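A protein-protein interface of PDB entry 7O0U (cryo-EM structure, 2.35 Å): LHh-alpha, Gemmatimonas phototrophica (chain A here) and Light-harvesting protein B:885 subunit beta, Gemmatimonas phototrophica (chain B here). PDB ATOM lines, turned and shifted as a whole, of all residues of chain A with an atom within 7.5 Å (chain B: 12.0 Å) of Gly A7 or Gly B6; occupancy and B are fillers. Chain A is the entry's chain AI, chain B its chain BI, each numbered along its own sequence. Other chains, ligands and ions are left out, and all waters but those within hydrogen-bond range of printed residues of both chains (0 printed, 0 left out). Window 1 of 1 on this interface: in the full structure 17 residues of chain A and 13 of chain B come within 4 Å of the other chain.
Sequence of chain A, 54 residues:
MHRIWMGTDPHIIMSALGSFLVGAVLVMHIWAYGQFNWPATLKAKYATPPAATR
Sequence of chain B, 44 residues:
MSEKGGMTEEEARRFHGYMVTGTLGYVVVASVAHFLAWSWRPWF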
ATOM      1  N   ARG A   3      28.608   4.045 -12.683  1.00  0.00           N
ATOM      2  CA  ARG A   3      28.274   2.638 -12.887  1.00  0.00           C
ATOM      3  C   ARG A   3      27.914   1.911 -11.596  1.00  0.00           C
ATOM      4  O   ARG A   3      27.256   0.866 -11.655  1.00  0.00           O
ATOM      5  CB  ARG A   3      29.436   1.924 -13.576  1.00  0.00           C
ATOM      6  CG  ARG A   3      29.667   2.377 -15.009  1.00  0.00           C
ATOM      7  CD  ARG A   3      30.879   1.695 -15.619  1.00  0.00           C
ATOM      8  NE  ARG A   3      31.171   2.193 -16.959  1.00  0.00           N
ATOM      9  CZ  ARG A   3      30.559   1.788 -18.063  1.00  0.00           C
ATOM     10  NH1 ARG A   3      29.608   0.870 -18.031  1.00  0.00           N
ATOM     11  NH2 ARG A   3      30.911   2.320 -19.230  1.00  0.00           N
ATOM     12  N   ILE A   4      28.336   2.423 -10.437  1.00  0.00           N
ATOM     13  CA  ILE A   4      27.970   1.800  -9.166  1.00  0.00           C
ATOM     14  C   ILE A   4      26.457   1.771  -8.976  1.00  0.00           C
ATOM     15  O   ILE A   4      25.922   0.849  -8.348  1.00  0.00           O
ATOM     16  CB  ILE A   4      28.686   2.512  -7.997  1.00  0.00           C
ATOM     17  CG1 ILE A   4      28.631   1.657  -6.728  1.00  0.00           C
ATOM     18  CG2 ILE A   4      28.092   3.890  -7.740  1.00  0.00           C
ATOM     19  CD1 ILE A   4      29.354   0.334  -6.850  1.00  0.00           C
ATOM     20  N   TRP A   5      25.743   2.759  -9.519  1.00  0.00           N
ATOM     21  CA  TRP A   5      24.289   2.799  -9.407  1.00  0.00           C
ATOM     22  C   TRP A   5      23.576   1.822 -10.334  1.00  0.00           C
ATOM     23  O   TRP A   5      22.379   1.583 -10.145  1.00  0.00           O
ATOM     24  CB  TRP A   5      23.776   4.213  -9.682  1.00  0.00           C
ATOM     25  CG  TRP A   5      24.533   5.302  -8.979  1.00  0.00           C
ATOM     26  CD1 TRP A   5      25.139   6.375  -9.560  1.00  0.00           C
ATOM     27  CD2 TRP A   5      24.750   5.438  -7.565  1.00  0.00           C
ATOM     28  NE1 TRP A   5      25.725   7.165  -8.604  1.00  0.00           N
ATOM     29  CE2 TRP A   5      25.502   6.614  -7.372  1.00  0.00           C
ATOM     30  CE3 TRP A   5      24.386   4.681  -6.447  1.00  0.00           C
ATOM     31  CZ2 TRP A   5      25.897   7.049  -6.109  1.00  0.00           C
ATOM     32  CZ3 TRP A   5      24.780   5.115  -5.193  1.00  0.00           C
ATOM     33  CH2 TRP A   5      25.526   6.288  -5.035  1.00  0.00           C
ATOM     34  N   MET A   6      24.260   1.276 -11.340  1.00  0.00           N
ATOM     35  CA  MET A   6      23.634   0.295 -12.218  1.00  0.00           C
ATOM     36  C   MET A   6      23.120  -0.898 -11.420  1.00  0.00           C
ATOM     37  O   MET A   6      23.682  -1.277 -10.389  1.00  0.00           O
ATOM     38  CB  MET A   6      24.622  -0.170 -13.291  1.00  0.00           C
ATOM     39  CG  MET A   6      25.046   0.931 -14.253  1.00  0.00           C
ATOM     40  SD  MET A   6      26.345   0.433 -15.402  1.00  0.00           S
ATOM     41  CE  MET A   6      25.492  -0.816 -16.362  1.00  0.00           C
ATOM     42  N   GLY A   7      22.034  -1.496 -11.910  1.00  0.00           N
ATOM     43  CA  GLY A   7      21.407  -2.613 -11.236  1.00  0.00           C
ATOM     44  C   GLY A   7      20.663  -2.272  -9.964  1.00  0.00           C
ATOM     45  O   GLY A   7      20.170  -3.186  -9.294  1.00  0.00           O
ATOM     46  N   THR A   8      20.564  -0.994  -9.607  1.00  0.00           N
ATOM     47  CA  THR A   8      20.044  -0.560  -8.318  1.00  0.00           C
ATOM     48  C   THR A   8      18.811   0.312  -8.526  1.00  0.00           C
ATOM     49  O   THR A   8      18.754   1.104  -9.471  1.00  0.00           O
ATOM     50  CB  THR A   8      21.108   0.211  -7.530  1.00  0.00           C
ATOM     51  OG1 THR A   8      22.372  -0.452  -7.663  1.00  0.00           O
ATOM     52  CG2 THR A   8      20.744   0.260  -6.060  1.00  0.00           C
ATOM     53  N   ASP A   9      17.824   0.156  -7.646  1.00  0.00           N
ATOM     54  CA  ASP A   9      16.636   1.008  -7.670  1.00  0.00           C
ATOM     55  C   ASP A   9      16.967   2.392  -7.111  1.00  0.00           C
ATOM     56  O   ASP A   9      17.620   2.490  -6.067  1.00  0.00           O
ATOM     57  CB  ASP A   9      15.520   0.344  -6.859  1.00  0.00           C
ATOM     58  CG  ASP A   9      14.439   1.313  -6.418  1.00  0.00           C
ATOM     59  OD1 ASP A   9      13.986   2.134  -7.239  1.00  0.00           O
ATOM     60  OD2 ASP A   9      14.037   1.244  -5.237  1.00  0.00           O
ATOM     61  N   PRO A  10      16.546   3.475  -7.776  1.00  0.00           N
ATOM     62  CA  PRO A  10      16.755   4.819  -7.203  1.00  0.00           C
ATOM     63  C   PRO A  10      16.111   5.034  -5.843  1.00  0.00           C
ATOM     64  O   PRO A  10      16.686   5.721  -4.991  1.00  0.00           O
ATOM     65  CB  PRO A  10      16.146   5.750  -8.263  1.00  0.00           C
ATOM     66  CG  PRO A  10      16.223   4.979  -9.531  1.00  0.00           C
ATOM     67  CD  PRO A  10      16.006   3.541  -9.143  1.00  0.00           C
ATOM     68  N   ILE A  13      17.844   3.610  -2.780  1.00  0.00           N
ATOM     69  CA  ILE A  13      19.017   4.442  -2.505  1.00  0.00           C
ATOM     70  C   ILE A  13      18.621   5.692  -1.730  1.00  0.00           C
ATOM     71  O   ILE A  13      19.199   6.004  -0.682  1.00  0.00           O
ATOM     72  CB  ILE A  13      19.748   4.814  -3.807  1.00  0.00           C
ATOM     73  CG1 ILE A  13      20.339   3.581  -4.485  1.00  0.00           C
ATOM     74  CG2 ILE A  13      20.839   5.838  -3.527  1.00  0.00           C
ATOM     75  CD1 ILE A  13      20.654   3.810  -5.943  1.00  0.00           C
ATOM     76  N   GLY B   5      17.441  -5.991 -13.751  1.00  0.00           N
ATOM     77  CA  GLY B   5      16.799  -5.166 -12.744  1.00  0.00           C
ATOM     78  C   GLY B   5      17.533  -3.866 -12.474  1.00  0.00           C
ATOM     79  O   GLY B   5      18.694  -3.709 -12.848  1.00  0.00           O
ATOM     80  N   GLY B   6      16.851  -2.935 -11.814  1.00  0.00           N
ATOM     81  CA  GLY B   6      17.384  -1.637 -11.456  1.00  0.00           C
ATOM     82  C   GLY B   6      17.792  -0.764 -12.639  1.00  0.00           C
ATOM     83  O   GLY B   6      17.412  -0.986 -13.791  1.00  0.00           O
ATOM     84  N   MET B   7      18.588   0.256 -12.315  1.00  0.00           N
ATOM     85  CA  MET B   7      18.994   1.263 -13.289  1.00  0.00           C
ATOM     86  C   MET B   7      19.847   0.687 -14.415  1.00  0.00           C
ATOM     87  O   MET B   7      20.742  -0.133 -14.193  1.00  0.00           O
ATOM     88  CB  MET B   7      19.746   2.395 -12.591  1.00  0.00           C
ATOM     89  CG  MET B   7      18.835   3.352 -11.846  1.00  0.00           C
ATOM     90  SD  MET B   7      19.715   4.747 -11.130  1.00  0.00           S
ATOM     91  CE  MET B   7      20.066   4.107  -9.497  1.00  0.00           C
ATOM     92  N   THR B   8      19.551   1.135 -15.634  1.00  0.00           N
ATOM     93  CA  THR B   8      20.457   1.065 -16.773  1.00  0.00           C
ATOM     94  C   THR B   8      21.676   1.971 -16.572  1.00  0.00           C
ATOM     95  O   THR B   8      21.748   2.776 -15.640  1.00  0.00           O
ATOM     96  CB  THR B   8      19.731   1.470 -18.054  1.00  0.00           C
ATOM     97  OG1 THR B   8      19.219   2.801 -17.907  1.00  0.00           O
ATOM     98  CG2 THR B   8      18.577   0.523 -18.336  1.00  0.00           C
ATOM     99  N   GLU B   9      22.646   1.814 -17.478  1.00  0.00           N
ATOM    100  CA  GLU B   9      23.755   2.761 -17.602  1.00  0.00           C
ATOM    101  C   GLU B   9      23.281   4.207 -17.694  1.00  0.00           C
ATOM    102  O   GLU B   9      23.839   5.093 -17.035  1.00  0.00           O
ATOM    103  CB  GLU B   9      24.595   2.396 -18.833  1.00  0.00           C
ATOM    104  CG  GLU B   9      25.389   3.538 -19.480  1.00  0.00           C
ATOM    105  CD  GLU B   9      26.454   4.143 -18.584  1.00  0.00           C
ATOM    106  OE1 GLU B   9      26.913   3.460 -17.647  1.00  0.00           O
ATOM    107  OE2 GLU B   9      26.849   5.303 -18.835  1.00  0.00           O
ATOM    108  N   GLU B  10      22.255   4.471 -18.503  1.00  0.00           N
ATOM    109  CA  GLU B  10      21.838   5.854 -18.728  1.00  0.00           C
ATOM    110  C   GLU B  10      21.072   6.432 -17.544  1.00  0.00           C
ATOM    111  O   GLU B  10      21.216   7.621 -17.236  1.00  0.00           O
ATOM    112  CB  GLU B  10      21.011   5.956 -20.008  1.00  0.00           C
ATOM    113  CG  GLU B  10      21.845   5.844 -21.274  1.00  0.00           C
ATOM    114  CD  GLU B  10      22.888   6.945 -21.386  1.00  0.00           C
ATOM    115  OE1 GLU B  10      22.652   8.054 -20.858  1.00  0.00           O
ATOM    116  OE2 GLU B  10      23.948   6.702 -22.000  1.00  0.00           O
ATOM    117  N   GLU B  11      20.256   5.624 -16.867  1.00  0.00           N
ATOM    118  CA  GLU B  11      19.672   6.076 -15.607  1.00  0.00           C
ATOM    119  C   GLU B  11      20.759   6.325 -14.568  1.00  0.00           C
ATOM    120  O   GLU B  11      20.773   7.367 -13.904  1.00  0.00           O
ATOM    121  CB  GLU B  11      18.659   5.050 -15.099  1.00  0.00           C
ATOM    122  CG  GLU B  11      17.395   4.961 -15.938  1.00  0.00           C
ATOM    123  CD  GLU B  11      16.683   3.632 -15.779  1.00  0.00           C
ATOM    124  OE1 GLU B  11      17.324   2.583 -15.998  1.00  0.00           O
ATOM    125  OE2 GLU B  11      15.479   3.636 -15.442  1.00  0.00           O
ATOM    126  N   ALA B  12      21.682   5.373 -14.421  1.00  0.00           N
ATOM    127  CA  ALA B  12      22.812   5.540 -13.510  1.00  0.00           C
ATOM    128  C   ALA B  12      23.614   6.799 -13.825  1.00  0.00           C
ATOM    129  O   ALA B  12      24.056   7.507 -12.913  1.00  0.00           O
ATOM    130  CB  ALA B  12      23.710   4.306 -13.561  1.00  0.00           C
ATOM    131  N   ARG B  13      23.816   7.088 -15.113  1.00  0.00           N
ATOM    132  CA  ARG B  13      24.497   8.314 -15.520  1.00  0.00           C
ATOM    133  C   ARG B  13      23.763   9.559 -15.030  1.00  0.00           C
ATOM    134  O   ARG B  13      24.360  10.439 -14.400  1.00  0.00           O
ATOM    135  CB  ARG B  13      24.629   8.336 -17.044  1.00  0.00           C
ATOM    136  CG  ARG B  13      25.434   9.491 -17.612  1.00  0.00           C
ATOM    137  CD  ARG B  13      26.923   9.285 -17.397  1.00  0.00           C
ATOM    138  NE  ARG B  13      27.433   8.209 -18.237  1.00  0.00           N
ATOM    139  CZ  ARG B  13      28.579   8.250 -18.904  1.00  0.00           C
ATOM    140  NH1 ARG B  13      29.379   9.300 -18.837  1.00  0.00           N
ATOM    141  NH2 ARG B  13      28.932   7.209 -19.651  1.00  0.00           N
ATOM    142  N   ARG B  14      22.464   9.653 -15.317  1.00  0.00           N
ATOM    143  CA  ARG B  14      21.690  10.831 -14.932  1.00  0.00           C
ATOM    144  C   ARG B  14      21.540  10.928 -13.417  1.00  0.00           C
ATOM    145  O   ARG B  14      21.700  12.006 -12.832  1.00  0.00           O
ATOM    146  CB  ARG B  14      20.325  10.805 -15.623  1.00  0.00           C
ATOM    147  CG  ARG B  14      19.671  12.173 -15.751  1.00  0.00           C
ATOM    148  CD  ARG B  14      18.208  12.099 -16.196  1.00  0.00           C
ATOM    149  NE  ARG B  14      18.038  11.434 -17.484  1.00  0.00           N
ATOM    150  CZ  ARG B  14      17.767  10.146 -17.648  1.00  0.00           C
ATOM    151  NH1 ARG B  14      17.463   9.367 -16.624  1.00  0.00           N
ATOM    152  NH2 ARG B  14      17.755   9.637 -18.877  1.00  0.00           N
ATOM    153  N   PHE B  15      21.223   9.805 -12.772  1.00  0.00           N
ATOM    154  CA  PHE B  15      21.099   9.748 -11.317  1.00  0.00           C
ATOM    155  C   PHE B  15      22.367  10.234 -10.620  1.00  0.00           C
ATOM    156  O   PHE B  15      22.302  11.013  -9.662  1.00  0.00           O
ATOM    157  CB  PHE B  15      20.763   8.313 -10.904  1.00  0.00           C
ATOM    158  CG  PHE B  15      20.581   8.116  -9.427  1.00  0.00           C
ATOM    159  CD1 PHE B  15      19.341   8.301  -8.841  1.00  0.00           C
ATOM    160  CD2 PHE B  15      21.639   7.708  -8.632  1.00  0.00           C
ATOM    161  CE1 PHE B  15      19.163   8.107  -7.486  1.00  0.00           C
ATOM    162  CE2 PHE B  15      21.467   7.512  -7.276  1.00  0.00           C
ATOM    163  CZ  PHE B  15      20.227   7.711  -6.704  1.00  0.00           C
ATOM    164  N   HIS B  16      23.531   9.777 -11.086  1.00  0.00           N
ATOM    165  CA  HIS B  16      24.805  10.205 -10.508  1.00  0.00           C
ATOM    166  C   HIS B  16      25.001  11.717 -10.555  1.00  0.00           C
ATOM    167  O   HIS B  16      25.468  12.312  -9.577  1.00  0.00           O
ATOM    168  CB  HIS B  16      25.957   9.515 -11.232  1.00  0.00           C
ATOM    169  CG  HIS B  16      27.295   9.756 -10.608  1.00  0.00           C
ATOM    170  ND1 HIS B  16      27.665   9.221  -9.394  1.00  0.00           N
ATOM    171  CD2 HIS B  16      28.354  10.484 -11.035  1.00  0.00           C
ATOM    172  CE1 HIS B  16      28.894   9.607  -9.101  1.00  0.00           C
ATOM    173  NE2 HIS B  16      29.334  10.375 -10.081  1.00  0.00           N
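Printed residues of chain B that touch a printed residue of chain A: Gly B5, Gly B6, Met B7, Glu B9, Ala B12, Phe B15 and His B16.
Hydrophobic or aromatic side chains of chain B within 4 Å of the printed part of chain A: Met B7, Ala B12, Phe B15 and His B16.
Of the 9 printed residues of chain A, 7 touch a printed residue of chain B.
Among the printed residues, Asp or Glu carboxylates within 4 Å of a Lys or Arg side-chain nitrogen of the other chain: Arg A3 with Glu B9 (3.8 Å).
The backbone NH (N) of Gly A7 lies within hydrogen-bond range of the backbone carbonyl oxygen (O) of Met B7.
NH1 of Arg A3 lies within salt-bridge range of OE1 of Glu B9, 3.8 Å away.
The indole nitrogen of Trp A5 is in hydrogen-bond range of a ring nitrogen (ND1) of His B16 (2.9 Å).
The backbone NH (N) of Met B7 sits at hydrogen-bond distance from the backbone carbonyl oxygen (O) of Thr A8 (3.0 Å).
O of Met A6 is in hydrogen-bond range of OG1 of Thr A8 (3.1 Å).
The side-chain carboxylate (OE2) of Glu B9 is in salt-bridge range of the guanidinium group (NH2) of Arg B13 (2.9 Å).
O of Trp A5 sits at hydrogen-bond distance from OG1 of Thr A8, at 3.2 Å.
Of chain B, only Gly B5, Gly B6 and Met B7 come within 4 Å of Gly A7.
Gly B6 touches two residues of chain A.
Of chain B, only Gly B6 (3.7 Å) and Met B7 (3.0 Å) come within 4 Å of Thr A8.
Of the printed residues of chain A, Phe B15 touches Trp A5, Pro A10 and Ile A13.
Of the printed residues of chain B, Arg A3 touches Glu B9 (3.8 Å).
Of the printed residues of chain B, Pro A10 touches Met B7 and Phe B15.
Of the printed residues of chain A, His B16 touches Trp A5.
Glu B11 touches none of the printed residues of chain A.
The nearest residue of chain B that does not touch Gly A7 is Thr B8 (5.2 Å).
Among the printed residues, pairs that only touch across the chains: Gly A7 with Gly B5 (3.3 Å), Trp A5 with Met B7 (3.5 Å), Met A6 with Met B7 (3.5 Å), Ile A13 with Met B7 (3.6 Å), Thr A8 with Gly B6 (3.7 Å), Gly A7 with Gly B6 (3.7 Å), Met A6 with Ala B12 (3.7 Å), Trp A5 with Ala B12 (3.7 Å), Ile A13 with Phe B15 (3.7 Å), Trp A5 with Phe B15 (3.8 Å), Met A6 with Glu B9 (3.8 Å), Pro A10 with Met B7 (3.8 Å) and Pro A10 with Phe B15 (3.9 Å).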
